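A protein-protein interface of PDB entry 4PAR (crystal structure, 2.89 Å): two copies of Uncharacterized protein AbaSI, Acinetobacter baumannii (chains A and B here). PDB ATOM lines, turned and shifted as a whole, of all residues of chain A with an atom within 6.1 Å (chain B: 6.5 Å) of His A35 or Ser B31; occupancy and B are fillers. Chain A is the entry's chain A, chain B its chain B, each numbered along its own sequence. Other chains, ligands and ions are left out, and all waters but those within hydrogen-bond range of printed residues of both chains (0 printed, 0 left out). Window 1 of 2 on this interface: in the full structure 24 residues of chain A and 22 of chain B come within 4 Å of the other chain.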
ATOM      1  N   LEU A  17       3.686  22.691 -15.243  1.00  0.00           N
ATOM      2  CA  LEU A  17       4.419  22.181 -16.394  1.00  0.00           C
ATOM      3  C   LEU A  17       3.614  21.102 -17.115  1.00  0.00           C
ATOM      4  O   LEU A  17       4.073  20.508 -18.094  1.00  0.00           O
ATOM      5  CB  LEU A  17       5.779  21.641 -15.960  1.00  0.00           C
ATOM      6  CG  LEU A  17       6.660  22.677 -15.268  1.00  0.00           C
ATOM      7  CD1 LEU A  17       7.962  22.079 -14.798  1.00  0.00           C
ATOM      8  CD2 LEU A  17       6.925  23.845 -16.188  1.00  0.00           C
ATOM      9  N   VAL A  30      10.171  26.076 -21.722  1.00  0.00           N
ATOM     10  CA  VAL A  30       9.832  26.379 -20.342  1.00  0.00           C
ATOM     11  C   VAL A  30      10.433  25.351 -19.393  1.00  0.00           C
ATOM     12  O   VAL A  30      11.079  25.712 -18.404  1.00  0.00           O
ATOM     13  CB  VAL A  30       8.314  26.451 -20.139  1.00  0.00           C
ATOM     14  CG1 VAL A  30       7.979  26.605 -18.657  1.00  0.00           C
ATOM     15  CG2 VAL A  30       7.734  27.609 -20.958  1.00  0.00           C
ATOM     16  N   SER A  31      10.238  24.071 -19.695  1.00  0.00           N
ATOM     17  CA  SER A  31      10.734  23.031 -18.800  1.00  0.00           C
ATOM     18  C   SER A  31      12.251  23.133 -18.677  1.00  0.00           C
ATOM     19  O   SER A  31      12.803  23.000 -17.575  1.00  0.00           O
ATOM     20  CB  SER A  31      10.322  21.640 -19.282  1.00  0.00           C
ATOM     21  OG  SER A  31      10.931  21.323 -20.520  1.00  0.00           O
ATOM     22  N   ARG A  32      12.927  23.408 -19.791  1.00  0.00           N
ATOM     23  CA  ARG A  32      14.379  23.513 -19.732  1.00  0.00           C
ATOM     24  C   ARG A  32      14.800  24.724 -18.897  1.00  0.00           C
ATOM     25  O   ARG A  32      15.739  24.630 -18.101  1.00  0.00           O
ATOM     26  CB  ARG A  32      15.003  23.585 -21.127  1.00  0.00           C
ATOM     27  CG  ARG A  32      16.522  23.582 -21.059  1.00  0.00           C
ATOM     28  CD  ARG A  32      17.186  23.489 -22.413  1.00  0.00           C
ATOM     29  NE  ARG A  32      18.617  23.762 -22.310  1.00  0.00           N
ATOM     30  CZ  ARG A  32      19.548  22.838 -22.101  1.00  0.00           C
ATOM     31  NH1 ARG A  32      19.208  21.559 -21.972  1.00  0.00           N
ATOM     32  NH2 ARG A  32      20.823  23.191 -22.021  1.00  0.00           N
ATOM     33  N   ILE A  33      14.103  25.848 -19.060  1.00  0.00           N
ATOM     34  CA  ILE A  33      14.395  27.033 -18.248  1.00  0.00           C
ATOM     35  C   ILE A  33      14.270  26.721 -16.763  1.00  0.00           C
ATOM     36  O   ILE A  33      15.186  26.988 -15.983  1.00  0.00           O
ATOM     37  CB  ILE A  33      13.463  28.219 -18.575  1.00  0.00           C
ATOM     38  CG1 ILE A  33      13.809  28.815 -19.937  1.00  0.00           C
ATOM     39  CG2 ILE A  33      13.570  29.305 -17.503  1.00  0.00           C
ATOM     40  CD1 ILE A  33      12.948  29.986 -20.309  1.00  0.00           C
ATOM     41  N   ILE A  34      13.138  26.141 -16.377  1.00  0.00           N
ATOM     42  CA  ILE A  34      12.913  25.816 -14.977  1.00  0.00           C
ATOM     43  C   ILE A  34      13.961  24.860 -14.424  1.00  0.00           C
ATOM     44  O   ILE A  34      14.568  25.148 -13.392  1.00  0.00           O
ATOM     45  CB  ILE A  34      11.537  25.208 -14.760  1.00  0.00           C
ATOM     46  CG1 ILE A  34      10.469  26.192 -15.223  1.00  0.00           C
ATOM     47  CG2 ILE A  34      11.341  24.894 -13.290  1.00  0.00           C
ATOM     48  CD1 ILE A  34      10.526  27.519 -14.488  1.00  0.00           C
ATOM     49  N   HIS A  35      14.184  23.737 -15.102  1.00  0.00           N
ATOM     50  CA  HIS A  35      15.116  22.733 -14.580  1.00  0.00           C
ATOM     51  C   HIS A  35      16.550  23.239 -14.517  1.00  0.00           C
ATOM     52  O   HIS A  35      17.266  22.938 -13.572  1.00  0.00           O
ATOM     53  CB  HIS A  35      15.068  21.452 -15.413  1.00  0.00           C
ATOM     54  CG  HIS A  35      13.770  20.721 -15.313  1.00  0.00           C
ATOM     55  ND1 HIS A  35      13.249  19.984 -16.354  1.00  0.00           N
ATOM     56  CD2 HIS A  35      12.878  20.626 -14.299  1.00  0.00           C
ATOM     57  CE1 HIS A  35      12.091  19.466 -15.986  1.00  0.00           C
ATOM     58  NE2 HIS A  35      11.844  19.839 -14.743  1.00  0.00           N
ATOM     59  N   LEU A  36      16.975  23.996 -15.522  1.00  0.00           N
ATOM     60  CA  LEU A  36      18.344  24.501 -15.539  1.00  0.00           C
ATOM     61  C   LEU A  36      18.517  25.619 -14.516  1.00  0.00           C
ATOM     62  O   LEU A  36      19.609  25.823 -13.984  1.00  0.00           O
ATOM     63  CB  LEU A  36      18.725  24.992 -16.934  1.00  0.00           C
ATOM     64  CG  LEU A  36      19.395  23.994 -17.880  1.00  0.00           C
ATOM     65  CD1 LEU A  36      18.529  22.771 -18.097  1.00  0.00           C
ATOM     66  CD2 LEU A  36      19.710  24.670 -19.206  1.00  0.00           C
ATOM     67  N   LEU A  37      17.444  26.358 -14.258  1.00  0.00           N
ATOM     68  CA  LEU A  37      17.443  27.309 -13.156  1.00  0.00           C
ATOM     69  C   LEU A  37      17.382  26.577 -11.818  1.00  0.00           C
ATOM     70  O   LEU A  37      18.234  26.770 -10.958  1.00  0.00           O
ATOM     71  CB  LEU A  37      16.263  28.275 -13.287  1.00  0.00           C
ATOM     72  CG  LEU A  37      15.895  29.176 -12.105  1.00  0.00           C
ATOM     73  CD1 LEU A  37      17.076  30.021 -11.649  1.00  0.00           C
ATOM     74  CD2 LEU A  37      14.720  30.064 -12.476  1.00  0.00           C
ATOM     75  N   ASN A  38      16.348  25.752 -11.670  1.00  0.00           N
ATOM     76  CA  ASN A  38      16.061  24.930 -10.484  1.00  0.00           C
ATOM     77  C   ASN A  38      16.285  25.657  -9.140  1.00  0.00           C
ATOM     78  O   ASN A  38      16.797  25.097  -8.171  1.00  0.00           O
ATOM     79  CB  ASN A  38      16.811  23.573 -10.573  1.00  0.00           C
ATOM     80  CG  ASN A  38      18.201  23.576  -9.961  1.00  0.00           C
ATOM     81  OD1 ASN A  38      18.640  22.614  -9.345  1.00  0.00           O
ATOM     82  ND2 ASN A  38      18.897  24.696 -10.126  1.00  0.00           N
ATOM     83  N   PHE A  40      13.755  27.061  -6.507  1.00  0.00           N
ATOM     84  CA  PHE A  40      12.331  27.045  -6.198  1.00  0.00           C
ATOM     85  C   PHE A  40      11.930  28.041  -5.115  1.00  0.00           C
ATOM     86  O   PHE A  40      10.775  28.086  -4.698  1.00  0.00           O
ATOM     87  CB  PHE A  40      11.904  25.626  -5.848  1.00  0.00           C
ATOM     88  CG  PHE A  40      11.939  24.704  -7.029  1.00  0.00           C
ATOM     89  CD1 PHE A  40      13.090  24.001  -7.341  1.00  0.00           C
ATOM     90  CD2 PHE A  40      10.840  24.589  -7.863  1.00  0.00           C
ATOM     91  CE1 PHE A  40      13.132  23.171  -8.444  1.00  0.00           C
ATOM     92  CE2 PHE A  40      10.877  23.763  -8.966  1.00  0.00           C
ATOM     93  CZ  PHE A  40      12.025  23.054  -9.257  1.00  0.00           C
ATOM     94  N   LEU B  17       9.810  14.506 -26.705  1.00  0.00           N
ATOM     95  CA  LEU B  17       9.346  15.013 -25.411  1.00  0.00           C
ATOM     96  C   LEU B  17       7.930  15.597 -25.507  1.00  0.00           C
ATOM     97  O   LEU B  17       7.378  16.110 -24.529  1.00  0.00           O
ATOM     98  CB  LEU B  17      10.318  16.051 -24.854  1.00  0.00           C
ATOM     99  CG  LEU B  17      11.782  15.620 -24.803  1.00  0.00           C
ATOM    100  CD1 LEU B  17      12.629  16.618 -24.048  1.00  0.00           C
ATOM    101  CD2 LEU B  17      11.923  14.243 -24.195  1.00  0.00           C
ATOM    102  N   GLU B  26       5.439  11.557 -15.696  1.00  0.00           N
ATOM    103  CA  GLU B  26       6.349  11.202 -16.784  1.00  0.00           C
ATOM    104  C   GLU B  26       7.078  12.408 -17.385  1.00  0.00           C
ATOM    105  O   GLU B  26       8.315  12.467 -17.369  1.00  0.00           O
ATOM    106  CB  GLU B  26       5.574  10.475 -17.883  1.00  0.00           C
ATOM    107  CG  GLU B  26       6.397  10.085 -19.089  1.00  0.00           C
ATOM    108  CD  GLU B  26       5.525   9.641 -20.242  1.00  0.00           C
ATOM    109  OE1 GLU B  26       4.284   9.613 -20.062  1.00  0.00           O
ATOM    110  OE2 GLU B  26       6.078   9.328 -21.321  1.00  0.00           O
ATOM    111  N   ALA B  27       6.300  13.366 -17.893  1.00  0.00           N
ATOM    112  CA  ALA B  27       6.823  14.540 -18.602  1.00  0.00           C
ATOM    113  C   ALA B  27       7.907  15.272 -17.830  1.00  0.00           C
ATOM    114  O   ALA B  27       8.965  15.598 -18.378  1.00  0.00           O
ATOM    115  CB  ALA B  27       5.698  15.496 -18.920  1.00  0.00           C
ATOM    116  N   TYR B  28       7.626  15.518 -16.554  1.00  0.00           N
ATOM    117  CA  TYR B  28       8.544  16.200 -15.657  1.00  0.00           C
ATOM    118  C   TYR B  28       9.864  15.461 -15.494  1.00  0.00           C
ATOM    119  O   TYR B  28      10.939  16.027 -15.704  1.00  0.00           O
ATOM    120  CB  TYR B  28       7.897  16.377 -14.288  1.00  0.00           C
ATOM    121  CG  TYR B  28       8.751  17.173 -13.336  1.00  0.00           C
ATOM    122  CD1 TYR B  28       8.746  18.560 -13.375  1.00  0.00           C
ATOM    123  CD2 TYR B  28       9.569  16.543 -12.408  1.00  0.00           C
ATOM    124  CE1 TYR B  28       9.524  19.298 -12.525  1.00  0.00           C
ATOM    125  CE2 TYR B  28      10.357  17.280 -11.547  1.00  0.00           C
ATOM    126  CZ  TYR B  28      10.327  18.660 -11.613  1.00  0.00           C
ATOM    127  OH  TYR B  28      11.101  19.413 -10.765  1.00  0.00           O
ATOM    128  N   VAL B  29       9.766  14.194 -15.100  1.00  0.00           N
ATOM    129  CA  VAL B  29      10.933  13.374 -14.790  1.00  0.00           C
ATOM    130  C   VAL B  29      11.823  13.169 -16.010  1.00  0.00           C
ATOM    131  O   VAL B  29      13.042  13.358 -15.939  1.00  0.00           O
ATOM    132  CB  VAL B  29      10.516  12.004 -14.230  1.00  0.00           C
ATOM    133  CG1 VAL B  29      11.714  11.076 -14.131  1.00  0.00           C
ATOM    134  CG2 VAL B  29       9.841  12.171 -12.873  1.00  0.00           C
ATOM    135  N   VAL B  30      11.220  12.797 -17.132  1.00  0.00           N
ATOM    136  CA  VAL B  30      11.997  12.614 -18.354  1.00  0.00           C
ATOM    137  C   VAL B  30      12.611  13.932 -18.854  1.00  0.00           C
ATOM    138  O   VAL B  30      13.793  13.966 -19.226  1.00  0.00           O
ATOM    139  CB  VAL B  30      11.142  11.988 -19.463  1.00  0.00           C
ATOM    140  CG1 VAL B  30      11.920  11.938 -20.776  1.00  0.00           C
ATOM    141  CG2 VAL B  30      10.705  10.603 -19.044  1.00  0.00           C
ATOM    142  N   SER B  31      11.830  15.015 -18.851  1.00  0.00           N
ATOM    143  CA  SER B  31      12.368  16.294 -19.313  1.00  0.00           C
ATOM    144  C   SER B  31      13.528  16.739 -18.425  1.00  0.00           C
ATOM    145  O   SER B  31      14.526  17.281 -18.919  1.00  0.00           O
ATOM    146  CB  SER B  31      11.287  17.378 -19.356  1.00  0.00           C
ATOM    147  OG  SER B  31      10.782  17.653 -18.064  1.00  0.00           O
ATOM    148  N   ARG B  32      13.421  16.489 -17.123  1.00  0.00           N
ATOM    149  CA  ARG B  32      14.497  16.901 -16.237  1.00  0.00           C
ATOM    150  C   ARG B  32      15.731  16.039 -16.462  1.00  0.00           C
ATOM    151  O   ARG B  32      16.853  16.552 -16.463  1.00  0.00           O
ATOM    152  CB  ARG B  32      14.079  16.853 -14.769  1.00  0.00           C
ATOM    153  CG  ARG B  32      15.150  17.437 -13.850  1.00  0.00           C
ATOM    154  CD  ARG B  32      14.737  17.430 -12.395  1.00  0.00           C
ATOM    155  NE  ARG B  32      15.872  17.707 -11.519  1.00  0.00           N
ATOM    156  CZ  ARG B  32      16.227  18.921 -11.107  1.00  0.00           C
ATOM    157  NH1 ARG B  32      15.539  19.987 -11.485  1.00  0.00           N
ATOM    158  NH2 ARG B  32      17.277  19.067 -10.312  1.00  0.00           N
ATOM    159  N   ILE B  33      15.533  14.738 -16.669  1.00  0.00           N
ATOM    160  CA  ILE B  33      16.667  13.862 -16.960  1.00  0.00           C
ATOM    161  C   ILE B  33      17.396  14.326 -18.220  1.00  0.00           C
ATOM    162  O   ILE B  33      18.613  14.521 -18.198  1.00  0.00           O
ATOM    163  CB  ILE B  33      16.243  12.390 -17.130  1.00  0.00           C
ATOM    164  CG1 ILE B  33      15.815  11.804 -15.787  1.00  0.00           C
ATOM    165  CG2 ILE B  33      17.391  11.563 -17.682  1.00  0.00           C
ATOM    166  CD1 ILE B  33      15.182  10.451 -15.906  1.00  0.00           C
ATOM    167  N   ILE B  34      16.650  14.528 -19.304  1.00  0.00           N
ATOM    168  CA  ILE B  34      17.250  14.963 -20.566  1.00  0.00           C
ATOM    169  C   ILE B  34      17.980  16.295 -20.441  1.00  0.00           C
ATOM    170  O   ILE B  34      19.134  16.420 -20.859  1.00  0.00           O
ATOM    171  CB  ILE B  34      16.202  15.089 -21.673  1.00  0.00           C
ATOM    172  CG1 ILE B  34      15.624  13.719 -22.001  1.00  0.00           C
ATOM    173  CG2 ILE B  34      16.825  15.677 -22.921  1.00  0.00           C
ATOM    174  CD1 ILE B  34      16.669  12.726 -22.449  1.00  0.00           C
ATOM    175  N   HIS B  35      17.312  17.282 -19.855  1.00  0.00           N
ATOM    176  CA  HIS B  35      17.876  18.628 -19.778  1.00  0.00           C
ATOM    177  C   HIS B  35      19.097  18.707 -18.865  1.00  0.00           C
ATOM    178  O   HIS B  35      20.069  19.389 -19.182  1.00  0.00           O
ATOM    179  CB  HIS B  35      16.807  19.620 -19.314  1.00  0.00           C
ATOM    180  CG  HIS B  35      15.743  19.871 -20.336  1.00  0.00           C
ATOM    181  ND1 HIS B  35      14.416  20.048 -20.003  1.00  0.00           N
ATOM    182  CD2 HIS B  35      15.809  19.975 -21.684  1.00  0.00           C
ATOM    183  CE1 HIS B  35      13.710  20.246 -21.103  1.00  0.00           C
ATOM    184  NE2 HIS B  35      14.533  20.209 -22.137  1.00  0.00           N
ATOM    185  N   LEU B  36      19.051  18.004 -17.739  1.00  0.00           N
ATOM    186  CA  LEU B  36      20.177  18.005 -16.809  1.00  0.00           C
ATOM    187  C   LEU B  36      21.353  17.208 -17.358  1.00  0.00           C
ATOM    188  O   LEU B  36      22.507  17.590 -17.172  1.00  0.00           O
ATOM    189  CB  LEU B  36      19.760  17.444 -15.451  1.00  0.00           C
ATOM    190  CG  LEU B  36      19.278  18.444 -14.402  1.00  0.00           C
ATOM    191  CD1 LEU B  36      18.203  19.343 -14.969  1.00  0.00           C
ATOM    192  CD2 LEU B  36      18.767  17.713 -13.171  1.00  0.00           C
ATOM    193  N   HIS B 140      14.517  14.794  -7.247  1.00  0.00           N
ATOM    194  CA  HIS B 140      15.719  15.341  -7.858  1.00  0.00           C
ATOM    195  C   HIS B 140      16.949  14.511  -7.500  1.00  0.00           C
ATOM    196  O   HIS B 140      17.862  14.375  -8.316  1.00  0.00           O
ATOM    197  CB  HIS B 140      15.926  16.798  -7.437  1.00  0.00           C
ATOM    198  CG  HIS B 140      14.932  17.745  -8.030  1.00  0.00           C
ATOM    199  ND1 HIS B 140      15.106  19.112  -8.018  1.00  0.00           N
ATOM    200  CD2 HIS B 140      13.751  17.524  -8.657  1.00  0.00           C
ATOM    201  CE1 HIS B 140      14.078  19.691  -8.608  1.00  0.00           C
ATOM    202  NE2 HIS B 140      13.240  18.750  -9.004  1.00  0.00           N
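The guanidinium group (NH2) of Arg B32 sits at hydrogen-bond distance from a ring nitrogen (ND1) of His B140, 3.2 Å away.
The side-chain hydroxyl of Ser B31 is in hydrogen-bond range of the backbone carbonyl oxygen of Ala B27 (2.8 Å).
A ring nitrogen (ND1) of His B35 lies within hydrogen-bond range of the backbone carbonyl oxygen (O) of Ser B31, 3.0 Å away.
The backbone carbonyl oxygen (O) of Tyr B28 sits at hydrogen-bond distance from the side-chain hydroxyl (OG) of Ser B31 (2.9 Å).
NE2 of His B140 is in hydrogen-bond range of OH of Tyr B28, at 2.8 Å.
The backbone carbonyl oxygen (O) of Ser A31 is in hydrogen-bond range of a ring nitrogen (ND1) of His A35.
Among the printed residues, pairs that only touch across the chains: Ser A31 with His B35 (3.0 Å), His A35 with Ser B31 (3.1 Å), His A35 with Tyr B28 (3.3 Å), His A35 with Arg B32 (3.3 Å), Arg A32 with His B35 (3.5 Å), Phe A40 with His B140 (3.6 Å), Leu A36 with His B35 (3.8 Å), His A35 with Leu B36 (3.8 Å), His A35 with His B35 (3.8 Å), Leu A17 with Tyr B28 (3.9 Å) and Asn A38 with Arg B32 (3.9 Å).
Of chain A, only His A35 comes within 4 Å of Ser B31.
Of the printed residues of chain A, His B140 touches Phe A40.
Printed residues of chain B within 4 Å of Leu A17: Tyr B28.
Ile A34 touches none of the printed residues of chain B.
Ile B34 touches none of the printed residues of chain A.
The nearest residue of chain A that does not touch Ser B31 is Ser A31 (4.1 Å).
Hydrophobic or aromatic side chains of chain B that line the printed part of chain A: Tyr B28, His B35, Leu B36 and His B140.
Among the printed residues, 11 pairs touch across the chains.
Among the printed residues, no Asp or Glu carboxylate lies within 4 Å of a Lys or Arg side-chain nitrogen of the other chain.
Ser A31 touches His B35, and with the chains exchanged His A35 touches Ser B31.
Arg A32 touches His B35, and with the chains exchanged His A35 touches Arg B32.
His B35 touches its own counterpart, His A35.
His A35 touches Leu B36, and with the chains exchanged Leu A36 touches His B35.
Positions printed for both chains: 17, 30, 31, 32, 33, 34, 35 and 36.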
